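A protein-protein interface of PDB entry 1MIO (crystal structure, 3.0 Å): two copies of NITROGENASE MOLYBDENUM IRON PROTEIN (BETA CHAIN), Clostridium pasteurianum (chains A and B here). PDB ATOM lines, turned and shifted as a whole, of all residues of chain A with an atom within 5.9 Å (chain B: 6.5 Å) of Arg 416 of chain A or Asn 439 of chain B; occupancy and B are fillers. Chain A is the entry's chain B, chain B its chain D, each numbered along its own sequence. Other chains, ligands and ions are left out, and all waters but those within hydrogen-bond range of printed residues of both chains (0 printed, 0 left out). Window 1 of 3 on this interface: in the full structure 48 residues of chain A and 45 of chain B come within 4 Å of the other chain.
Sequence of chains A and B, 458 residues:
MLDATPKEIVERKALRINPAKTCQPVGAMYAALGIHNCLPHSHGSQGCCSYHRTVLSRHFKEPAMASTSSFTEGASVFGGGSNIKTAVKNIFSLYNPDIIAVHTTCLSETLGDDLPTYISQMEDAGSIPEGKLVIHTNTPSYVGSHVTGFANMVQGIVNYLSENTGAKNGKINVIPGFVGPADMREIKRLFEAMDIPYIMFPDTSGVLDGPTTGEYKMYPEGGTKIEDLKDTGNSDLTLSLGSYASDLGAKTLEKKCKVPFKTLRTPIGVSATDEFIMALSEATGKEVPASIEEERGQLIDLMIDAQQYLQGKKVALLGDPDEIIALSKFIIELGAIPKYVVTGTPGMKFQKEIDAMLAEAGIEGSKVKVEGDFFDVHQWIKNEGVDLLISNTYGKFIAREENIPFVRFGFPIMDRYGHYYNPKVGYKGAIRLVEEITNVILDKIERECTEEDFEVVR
NH2 of Arg 416 of chain A is in salt-bridge range of OE1 of Glu 446 of chain B (3.1 Å). The side-chain amino group (NZ) of Lys 61 of chain A is in salt-bridge range of the chain-end carboxylate (O) of Arg 458 of chain B (3.5 Å). OXT of Arg 458 of chain B is in hydrogen-bond range of OH of Tyr 417 of chain A, at 2.9 Å. NZ of Lys 396 of chain A is in salt-bridge range of OE2 of Glu 446 of chain B (2.8 Å). The side-chain carboxylate of Asp 443 of chain B is in salt-bridge range of the guanidinium group of Arg 416 of chain A, 3.4 Å away. The backbone carbonyl oxygen (O) of Met 414 of chain A sits close to the chain-end carboxylate (O) of Arg 458 of chain B, at 3.2 Å. The guanidinium group (NH2) of Arg 408 of chain A is in salt-bridge range of the side-chain carboxylate (OE1) of Glu 446 of chain B.
The side-chain amino group (NZ) of Lys 61 of chain A is in hydrogen-bond range of the backbone carbonyl oxygen (O) of Met 414 of chain A (3.5 Å). The side-chain carboxylate (OD2) of Asp 415 of chain A is in salt-bridge range of the side-chain amino group (NZ) of Lys 396 of chain A, at 2.9 Å. The side-chain carboxylate (OE2) of Glu 446 of chain B is in salt-bridge range of the guanidinium group (NE) of Arg 458 of chain B (3.2 Å). The side-chain amide nitrogen (ND2) of Asn 439 of chain B lies within hydrogen-bond range of the backbone carbonyl oxygen (O) of Glu 435 of chain B (3.2 Å). A ring nitrogen (NE2) of His 419 of chain A is in hydrogen-bond range of the backbone carbonyl oxygen (O) of His 59 of chain A (2.7 Å). OD1 of Asp 415 of chain A lies within salt-bridge range of NE of Arg 408 of chain A (2.8 Å).
Among the printed residues, pairs that only touch across the chains: Asp 415 of chain A with Leu 442 of chain B (3.4 Å), Asp 415 of chain A with Glu 446 of chain B (3.9 Å), Asp 415 of chain A with Arg 458 of chain B (3.4 Å), Arg 416 of chain A with Asn 439 of chain B (3.4 Å), Arg 416 of chain A with Leu 442 of chain B (3.7 Å), Tyr 417 of chain A with Glu 435 of chain B (3.7 Å), Tyr 417 of chain A with Thr 438 of chain B (3.8 Å), Gly 418 of chain A with Glu 435 of chain B (3.6 Å) and His 419 of chain A with Glu 435 of chain B (3.7 Å).
Arg 416 of chain A touches just these residues of chain B: Asn 439 (3.4 Å), Leu 442 (3.7 Å), Asp 443 (3.4 Å) and Glu 446 (3.1 Å). Printed residues of chain A within 4 Å of Asn 439 of chain B: Arg 416 (3.4 Å). Printed residues of chain B within 4 Å of His 419 of chain A: Glu 435 (3.7 Å). Printed residues of chain A within 4 Å of Arg 458 of chain B: Lys 61 (3.5 Å), Met 414 (3.2 Å), Asp 415 (3.4 Å) and Tyr 417 (2.9 Å). Of the printed residues of chain A, Thr 438 of chain B touches Tyr 417. Printed residues of chain A within 4 Å of Glu 446 of chain B: Lys 396 (2.8 Å), Arg 408 (3.5 Å), Asp 415 (3.9 Å) and Arg 416 (3.1 Å). Printed residues of chain B within 4 Å of Lys 396 of chain A: Glu 446. Val 434 of chain B touches none of the printed residues of chain A. The nearest residue of chain B that does not touch Arg 416 of chain A is Arg 458 of chain B (4.8 Å). The nearest residue of chain A that does not touch Asn 439 of chain B is Tyr 417 of chain A (4.2 Å).
Printed residues of chain A that touch a printed residue of chain B: Lys 61, Lys 396, Arg 408, Met 414, Asp 415, Arg 416, Tyr 417, Gly 418 and His 419. Along chain A the printed residues that touch a printed residue of chain B span positions 61 to 419. Of the 13 printed residues of chain B, 7 touch a printed residue of chain A. Printed residues of chain B that touch a printed residue of chain A: Glu 435, Thr 438, Asn 439, Leu 442, Asp 443, Glu 446 and Arg 458. Hydrophobic or aromatic side chains of chain B that line the printed part of chain A: Leu 442. Among the printed residues, 16 pairs touch across the chains. Among the printed residues, Asp or Glu carboxylates within 4 Å of a Lys or Arg side-chain nitrogen of the other chain: Lys 396 of chain A with Glu 446 of chain B, Arg 408 of chain A with Glu 446 of chain B, Arg 416 of chain A with Asp 443 of chain B and Arg 416 of chain A with Glu 446 of chain B.
1 position is printed for both chains. Of the 16 pairs that touch across the chains among the printed residues, none has its exchanged pair printed and touching as well.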
ATOM      1  N   HIS A  59     -18.065  15.731  -9.267  1.00  0.00           N
ATOM      2  CA  HIS A  59     -17.667  16.199  -7.942  1.00  0.00           C
ATOM      3  C   HIS A  59     -18.481  15.543  -6.840  1.00  0.00           C
ATOM      4  O   HIS A  59     -17.947  14.987  -5.883  1.00  0.00           O
ATOM      5  CB  HIS A  59     -17.861  17.700  -7.914  1.00  0.00           C
ATOM      6  CG  HIS A  59     -17.573  18.484  -6.634  1.00  0.00           C
ATOM      7  ND1 HIS A  59     -16.483  18.500  -5.875  1.00  0.00           N
ATOM      8  CD2 HIS A  59     -18.423  19.422  -6.112  1.00  0.00           C
ATOM      9  CE1 HIS A  59     -16.634  19.412  -4.942  1.00  0.00           C
ATOM     10  NE2 HIS A  59     -17.806  19.953  -5.098  1.00  0.00           N
ATOM     11  N   LYS A  61     -21.053  13.192  -7.443  1.00  0.00           N
ATOM     12  CA  LYS A  61     -21.532  11.879  -7.847  1.00  0.00           C
ATOM     13  C   LYS A  61     -23.066  11.883  -7.783  1.00  0.00           C
ATOM     14  O   LYS A  61     -23.734  11.104  -7.061  1.00  0.00           O
ATOM     15  CB  LYS A  61     -20.903  10.806  -6.928  1.00  0.00           C
ATOM     16  CG  LYS A  61     -19.487  10.363  -7.297  1.00  0.00           C
ATOM     17  CD  LYS A  61     -18.419  11.437  -7.170  1.00  0.00           C
ATOM     18  CE  LYS A  61     -17.026  11.007  -7.605  1.00  0.00           C
ATOM     19  NZ  LYS A  61     -16.893  10.962  -9.048  1.00  0.00           N
ATOM     20  N   LYS A 396      -3.020  17.205  -6.602  1.00  0.00           N
ATOM     21  CA  LYS A 396      -2.603  15.852  -6.290  1.00  0.00           C
ATOM     22  C   LYS A 396      -1.456  15.418  -7.134  1.00  0.00           C
ATOM     23  O   LYS A 396      -0.720  14.528  -6.728  1.00  0.00           O
ATOM     24  CB  LYS A 396      -3.746  14.871  -6.476  1.00  0.00           C
ATOM     25  CG  LYS A 396      -4.088  14.361  -7.847  1.00  0.00           C
ATOM     26  CD  LYS A 396      -5.365  13.663  -7.578  1.00  0.00           C
ATOM     27  CE  LYS A 396      -5.712  12.914  -8.795  1.00  0.00           C
ATOM     28  NZ  LYS A 396      -6.001  11.542  -8.429  1.00  0.00           N
ATOM     29  N   ARG A 408      -7.701  17.753   0.051  1.00  0.00           N
ATOM     30  CA  ARG A 408      -8.538  18.280  -1.011  1.00  0.00           C
ATOM     31  C   ARG A 408      -9.546  19.258  -0.446  1.00  0.00           C
ATOM     32  O   ARG A 408     -10.144  19.001   0.602  1.00  0.00           O
ATOM     33  CB  ARG A 408      -9.323  17.191  -1.669  1.00  0.00           C
ATOM     34  CG  ARG A 408      -8.591  16.177  -2.474  1.00  0.00           C
ATOM     35  CD  ARG A 408      -9.305  14.869  -2.318  1.00  0.00           C
ATOM     36  NE  ARG A 408      -8.765  13.928  -3.252  1.00  0.00           N
ATOM     37  CZ  ARG A 408      -7.534  13.447  -3.171  1.00  0.00           C
ATOM     38  NH1 ARG A 408      -6.691  13.774  -2.214  1.00  0.00           N
ATOM     39  NH2 ARG A 408      -7.100  12.668  -4.133  1.00  0.00           N
ATOM     40  N   ILE A 413     -13.287  18.399  -6.382  1.00  0.00           N
ATOM     41  CA  ILE A 413     -12.761  17.189  -5.779  1.00  0.00           C
ATOM     42  C   ILE A 413     -13.601  16.135  -6.463  1.00  0.00           C
ATOM     43  O   ILE A 413     -14.810  16.037  -6.227  1.00  0.00           O
ATOM     44  CB  ILE A 413     -13.020  17.219  -4.263  1.00  0.00           C
ATOM     45  CG1 ILE A 413     -12.357  18.426  -3.663  1.00  0.00           C
ATOM     46  CG2 ILE A 413     -12.535  15.942  -3.619  1.00  0.00           C
ATOM     47  CD1 ILE A 413     -13.271  18.774  -2.474  1.00  0.00           C
ATOM     48  N   MET A 414     -12.938  15.444  -7.361  1.00  0.00           N
ATOM     49  CA  MET A 414     -13.566  14.434  -8.184  1.00  0.00           C
ATOM     50  C   MET A 414     -13.084  13.000  -7.940  1.00  0.00           C
ATOM     51  O   MET A 414     -13.619  12.090  -8.574  1.00  0.00           O
ATOM     52  CB  MET A 414     -13.341  14.858  -9.620  1.00  0.00           C
ATOM     53  CG  MET A 414     -13.958  16.212 -10.003  1.00  0.00           C
ATOM     54  SD  MET A 414     -13.576  16.771 -11.692  1.00  0.00           S
ATOM     55  CE  MET A 414     -11.836  16.451 -11.691  1.00  0.00           C
ATOM     56  N   ASP A 415     -12.099  12.810  -7.026  1.00  0.00           N
ATOM     57  CA  ASP A 415     -11.499  11.513  -6.688  1.00  0.00           C
ATOM     58  C   ASP A 415     -12.147  10.721  -5.584  1.00  0.00           C
ATOM     59  O   ASP A 415     -11.839   9.541  -5.381  1.00  0.00           O
ATOM     60  CB  ASP A 415     -10.094  11.518  -6.146  1.00  0.00           C
ATOM     61  CG  ASP A 415      -9.265  12.652  -6.594  1.00  0.00           C
ATOM     62  OD1 ASP A 415      -9.337  13.700  -5.995  1.00  0.00           O
ATOM     63  OD2 ASP A 415      -8.547  12.493  -7.552  1.00  0.00           O
ATOM     64  N   ARG A 416     -12.973  11.339  -4.771  1.00  0.00           N
ATOM     65  CA  ARG A 416     -13.337  10.620  -3.581  1.00  0.00           C
ATOM     66  C   ARG A 416     -14.816  10.646  -3.416  1.00  0.00           C
ATOM     67  O   ARG A 416     -15.549  11.414  -4.074  1.00  0.00           O
ATOM     68  CB  ARG A 416     -12.677  11.230  -2.356  1.00  0.00           C
ATOM     69  CG  ARG A 416     -11.157  11.118  -2.243  1.00  0.00           C
ATOM     70  CD  ARG A 416     -10.609   9.702  -2.047  1.00  0.00           C
ATOM     71  NE  ARG A 416      -9.184   9.804  -1.819  1.00  0.00           N
ATOM     72  CZ  ARG A 416      -8.283   9.713  -2.796  1.00  0.00           C
ATOM     73  NH1 ARG A 416      -8.592   9.504  -4.087  1.00  0.00           N
ATOM     74  NH2 ARG A 416      -7.012   9.903  -2.469  1.00  0.00           N
ATOM     75  N   TYR A 417     -15.197   9.781  -2.475  1.00  0.00           N
ATOM     76  CA  TYR A 417     -16.587   9.587  -2.184  1.00  0.00           C
ATOM     77  C   TYR A 417     -16.831  10.200  -0.807  1.00  0.00           C
ATOM     78  O   TYR A 417     -15.931  10.413   0.000  1.00  0.00           O
ATOM     79  CB  TYR A 417     -16.858   8.050  -2.290  1.00  0.00           C
ATOM     80  CG  TYR A 417     -16.714   7.558  -3.740  1.00  0.00           C
ATOM     81  CD1 TYR A 417     -17.786   7.714  -4.611  1.00  0.00           C
ATOM     82  CD2 TYR A 417     -15.493   7.075  -4.234  1.00  0.00           C
ATOM     83  CE1 TYR A 417     -17.646   7.416  -5.954  1.00  0.00           C
ATOM     84  CE2 TYR A 417     -15.353   6.781  -5.576  1.00  0.00           C
ATOM     85  CZ  TYR A 417     -16.436   6.958  -6.417  1.00  0.00           C
ATOM     86  OH  TYR A 417     -16.356   6.669  -7.747  1.00  0.00           O
ATOM     87  N   GLY A 418     -18.047  10.687  -0.612  1.00  0.00           N
ATOM     88  CA  GLY A 418     -18.469  11.169   0.676  1.00  0.00           C
ATOM     89  C   GLY A 418     -18.133  12.605   0.983  1.00  0.00           C
ATOM     90  O   GLY A 418     -18.983  13.244   1.583  1.00  0.00           O
ATOM     91  N   HIS A 419     -17.004  13.184   0.558  1.00  0.00           N
ATOM     92  CA  HIS A 419     -16.630  14.567   0.895  1.00  0.00           C
ATOM     93  C   HIS A 419     -17.732  15.627   1.043  1.00  0.00           C
ATOM     94  O   HIS A 419     -17.811  16.442   1.953  1.00  0.00           O
ATOM     95  CB  HIS A 419     -15.593  15.078  -0.150  1.00  0.00           C
ATOM     96  CG  HIS A 419     -16.026  15.235  -1.619  1.00  0.00           C
ATOM     97  ND1 HIS A 419     -16.639  16.270  -2.176  1.00  0.00           N
ATOM     98  CD2 HIS A 419     -15.871  14.293  -2.617  1.00  0.00           C
ATOM     99  CE1 HIS A 419     -16.853  15.978  -3.429  1.00  0.00           C
ATOM    100  NE2 HIS A 419     -16.394  14.792  -3.700  1.00  0.00           N
ATOM    101  N   TYR A 420     -18.695  15.489   0.139  1.00  0.00           N
ATOM    102  CA  TYR A 420     -19.805  16.397  -0.129  1.00  0.00           C
ATOM    103  C   TYR A 420     -20.843  16.482   0.972  1.00  0.00           C
ATOM    104  O   TYR A 420     -21.589  17.458   0.982  1.00  0.00           O
ATOM    105  CB  TYR A 420     -20.430  15.964  -1.526  1.00  0.00           C
ATOM    106  CG  TYR A 420     -20.613  14.484  -1.875  1.00  0.00           C
ATOM    107  CD1 TYR A 420     -19.601  13.690  -2.384  1.00  0.00           C
ATOM    108  CD2 TYR A 420     -21.838  13.925  -1.678  1.00  0.00           C
ATOM    109  CE1 TYR A 420     -19.811  12.347  -2.678  1.00  0.00           C
ATOM    110  CE2 TYR A 420     -22.060  12.594  -1.976  1.00  0.00           C
ATOM    111  CZ  TYR A 420     -21.064  11.781  -2.478  1.00  0.00           C
ATOM    112  OH  TYR A 420     -21.389  10.441  -2.799  1.00  0.00           O
ATOM    113  N   GLU A 436      -8.303  16.179   9.687  1.00  0.00           N
ATOM    114  CA  GLU A 436      -7.688  15.699   8.462  1.00  0.00           C
ATOM    115  C   GLU A 436      -6.312  16.251   8.192  1.00  0.00           C
ATOM    116  O   GLU A 436      -5.515  15.473   7.700  1.00  0.00           O
ATOM    117  CB  GLU A 436      -8.580  15.997   7.265  1.00  0.00           C
ATOM    118  CG  GLU A 436      -8.176  15.212   5.971  1.00  0.00           C
ATOM    119  CD  GLU A 436      -8.802  13.851   5.561  1.00  0.00           C
ATOM    120  OE1 GLU A 436      -8.364  12.788   6.043  1.00  0.00           O
ATOM    121  OE2 GLU A 436      -9.701  13.869   4.704  1.00  0.00           O
ATOM    122  N   VAL B 434     -17.796   4.104   5.429  1.00  0.00           N
ATOM    123  CA  VAL B 434     -17.711   3.901   3.983  1.00  0.00           C
ATOM    124  C   VAL B 434     -16.676   4.866   3.398  1.00  0.00           C
ATOM    125  O   VAL B 434     -15.755   4.438   2.677  1.00  0.00           O
ATOM    126  CB  VAL B 434     -19.060   4.156   3.325  1.00  0.00           C
ATOM    127  CG1 VAL B 434     -18.980   3.924   1.834  1.00  0.00           C
ATOM    128  CG2 VAL B 434     -20.056   3.188   3.838  1.00  0.00           C
ATOM    129  N   GLU B 435     -16.800   6.153   3.777  1.00  0.00           N
ATOM    130  CA  GLU B 435     -15.856   7.177   3.381  1.00  0.00           C
ATOM    131  C   GLU B 435     -14.418   6.825   3.749  1.00  0.00           C
ATOM    132  O   GLU B 435     -13.594   6.894   2.844  1.00  0.00           O
ATOM    133  CB  GLU B 435     -16.259   8.504   4.017  1.00  0.00           C
ATOM    134  CG  GLU B 435     -15.157   9.587   4.058  1.00  0.00           C
ATOM    135  CD  GLU B 435     -15.579  11.033   3.766  1.00  0.00           C
ATOM    136  OE1 GLU B 435     -16.719  11.422   4.087  1.00  0.00           O
ATOM    137  OE2 GLU B 435     -14.752  11.766   3.195  1.00  0.00           O
ATOM    138  N   GLU B 436     -13.998   6.377   4.938  1.00  0.00           N
ATOM    139  CA  GLU B 436     -12.578   6.167   5.220  1.00  0.00           C
ATOM    140  C   GLU B 436     -12.055   4.894   4.706  1.00  0.00           C
ATOM    141  O   GLU B 436     -10.854   4.769   4.597  1.00  0.00           O
ATOM    142  CB  GLU B 436     -12.221   6.152   6.703  1.00  0.00           C
ATOM    143  CG  GLU B 436     -11.973   7.560   7.293  1.00  0.00           C
ATOM    144  CD  GLU B 436     -10.824   8.426   6.683  1.00  0.00           C
ATOM    145  OE1 GLU B 436      -9.751   7.896   6.310  1.00  0.00           O
ATOM    146  OE2 GLU B 436     -11.000   9.662   6.612  1.00  0.00           O
ATOM    147  N   ILE B 437     -12.957   3.964   4.430  1.00  0.00           N
ATOM    148  CA  ILE B 437     -12.591   2.686   3.854  1.00  0.00           C
ATOM    149  C   ILE B 437     -12.303   3.000   2.389  1.00  0.00           C
ATOM    150  O   ILE B 437     -11.226   2.666   1.930  1.00  0.00           O
ATOM    151  CB  ILE B 437     -13.767   1.671   4.049  1.00  0.00           C
ATOM    152  CG1 ILE B 437     -13.944   1.292   5.506  1.00  0.00           C
ATOM    153  CG2 ILE B 437     -13.477   0.418   3.228  1.00  0.00           C
ATOM    154  CD1 ILE B 437     -15.178   0.417   5.738  1.00  0.00           C
ATOM    155  N   THR B 438     -13.156   3.682   1.632  1.00  0.00           N
ATOM    156  CA  THR B 438     -12.871   4.083   0.273  1.00  0.00           C
ATOM    157  C   THR B 438     -11.580   4.892   0.154  1.00  0.00           C
ATOM    158  O   THR B 438     -10.778   4.667  -0.754  1.00  0.00           O
ATOM    159  CB  THR B 438     -14.121   4.836  -0.180  1.00  0.00           C
ATOM    160  OG1 THR B 438     -14.752   3.865  -0.989  1.00  0.00           O
ATOM    161  CG2 THR B 438     -13.924   6.169  -0.897  1.00  0.00           C
ATOM    162  N   ASN B 439     -11.303   5.822   1.059  1.00  0.00           N
ATOM    163  CA  ASN B 439     -10.119   6.646   0.985  1.00  0.00           C
ATOM    164  C   ASN B 439      -8.850   5.900   1.279  1.00  0.00           C
ATOM    165  O   ASN B 439      -7.894   6.129   0.566  1.00  0.00           O
ATOM    166  CB  ASN B 439     -10.115   7.775   1.956  1.00  0.00           C
ATOM    167  CG  ASN B 439     -11.068   8.930   1.790  1.00  0.00           C
ATOM    168  OD1 ASN B 439     -10.882   9.891   2.519  1.00  0.00           O
ATOM    169  ND2 ASN B 439     -12.093   8.974   0.947  1.00  0.00           N
ATOM    170  N   VAL B 440      -8.720   4.994   2.243  1.00  0.00           N
ATOM    171  CA  VAL B 440      -7.441   4.349   2.507  1.00  0.00           C
ATOM    172  C   VAL B 440      -6.962   3.426   1.387  1.00  0.00           C
ATOM    173  O   VAL B 440      -5.759   3.202   1.173  1.00  0.00           O
ATOM    174  CB  VAL B 440      -7.514   3.580   3.867  1.00  0.00           C
ATOM    175  CG1 VAL B 440      -7.893   4.651   4.854  1.00  0.00           C
ATOM    176  CG2 VAL B 440      -8.488   2.439   3.967  1.00  0.00           C
ATOM    177  N   ILE B 441      -7.976   2.920   0.673  1.00  0.00           N
ATOM    178  CA  ILE B 441      -7.853   2.059  -0.500  1.00  0.00           C
ATOM    179  C   ILE B 441      -7.356   2.879  -1.670  1.00  0.00           C
ATOM    180  O   ILE B 441      -6.264   2.593  -2.162  1.00  0.00           O
ATOM    181  CB  ILE B 441      -9.258   1.404  -0.699  1.00  0.00           C
ATOM    182  CG1 ILE B 441      -9.330   0.336   0.433  1.00  0.00           C
ATOM    183  CG2 ILE B 441      -9.509   0.846  -2.105  1.00  0.00           C
ATOM    184  CD1 ILE B 441     -10.596  -0.532   0.620  1.00  0.00           C
ATOM    185  N   LEU B 442      -8.116   3.928  -2.032  1.00  0.00           N
ATOM    186  CA  LEU B 442      -7.766   4.875  -3.085  1.00  0.00           C
ATOM    187  C   LEU B 442      -6.465   5.625  -2.818  1.00  0.00           C
ATOM    188  O   LEU B 442      -5.716   5.919  -3.754  1.00  0.00           O
ATOM    189  CB  LEU B 442      -8.882   5.874  -3.279  1.00  0.00           C
ATOM    190  CG  LEU B 442     -10.156   5.412  -3.917  1.00  0.00           C
ATOM    191  CD1 LEU B 442     -11.149   6.537  -4.012  1.00  0.00           C
ATOM    192  CD2 LEU B 442      -9.851   4.952  -5.304  1.00  0.00           C
ATOM    193  N   ASP B 443      -6.147   5.887  -1.545  1.00  0.00           N
ATOM    194  CA  ASP B 443      -4.862   6.422  -1.098  1.00  0.00           C
ATOM    195  C   ASP B 443      -3.758   5.469  -1.554  1.00  0.00           C
ATOM    196  O   ASP B 443      -2.841   5.918  -2.245  1.00  0.00           O
ATOM    197  CB  ASP B 443      -4.780   6.535   0.452  1.00  0.00           C
ATOM    198  CG  ASP B 443      -5.453   7.738   1.163  1.00  0.00           C
ATOM    199  OD1 ASP B 443      -6.088   8.516   0.445  1.00  0.00           O
ATOM    200  OD2 ASP B 443      -5.352   7.910   2.408  1.00  0.00           O
ATOM    201  N   LYS B 444      -3.846   4.161  -1.247  1.00  0.00           N
ATOM    202  CA  LYS B 444      -2.819   3.205  -1.619  1.00  0.00           C
ATOM    203  C   LYS B 444      -2.667   3.079  -3.116  1.00  0.00           C
ATOM    204  O   LYS B 444      -1.542   3.016  -3.615  1.00  0.00           O
ATOM    205  CB  LYS B 444      -3.110   1.827  -1.090  1.00  0.00           C
ATOM    206  CG  LYS B 444      -1.881   0.960  -1.294  1.00  0.00           C
ATOM    207  CD  LYS B 444      -2.126  -0.506  -1.011  1.00  0.00           C
ATOM    208  CE  LYS B 444      -0.922  -1.392  -1.313  1.00  0.00           C
ATOM    209  NZ  LYS B 444      -1.159  -2.737  -0.821  1.00  0.00           N
ATOM    210  N   GLU B 446      -3.396   5.345  -5.558  1.00  0.00           N
ATOM    211  CA  GLU B 446      -2.770   6.484  -6.162  1.00  0.00           C
ATOM    212  C   GLU B 446      -1.314   6.662  -5.794  1.00  0.00           C
ATOM    213  O   GLU B 446      -0.620   7.508  -6.340  1.00  0.00           O
ATOM    214  CB  GLU B 446      -3.563   7.687  -5.778  1.00  0.00           C
ATOM    215  CG  GLU B 446      -4.981   7.602  -6.296  1.00  0.00           C
ATOM    216  CD  GLU B 446      -5.781   8.882  -6.200  1.00  0.00           C
ATOM    217  OE1 GLU B 446      -5.654   9.621  -5.230  1.00  0.00           O
ATOM    218  OE2 GLU B 446      -6.533   9.135  -7.125  1.00  0.00           O
ATOM    219  N   ARG B 458     -11.747   9.471  -9.979  1.00  0.00           N
ATOM    220  CA  ARG B 458     -11.812   8.137  -9.477  1.00  0.00           C
ATOM    221  C   ARG B 458     -13.268   7.956  -9.089  1.00  0.00           C
ATOM    222  O   ARG B 458     -14.045   8.915  -9.068  1.00  0.00           O
ATOM    223  CB  ARG B 458     -10.933   8.001  -8.282  1.00  0.00           C
ATOM    224  CG  ARG B 458      -9.490   8.070  -8.620  1.00  0.00           C
ATOM    225  CD  ARG B 458      -8.942   6.670  -8.801  1.00  0.00           C
ATOM    226  NE  ARG B 458      -7.519   6.782  -9.064  1.00  0.00           N
ATOM    227  CZ  ARG B 458      -6.854   5.867  -9.771  1.00  0.00           C
ATOM    228  NH1 ARG B 458      -7.506   4.800 -10.242  1.00  0.00           N
ATOM    229  NH2 ARG B 458      -5.546   6.045 -10.054  1.00  0.00           N
ATOM    230  OXT ARG B 458     -13.623   6.820  -8.824  1.00  0.00           O
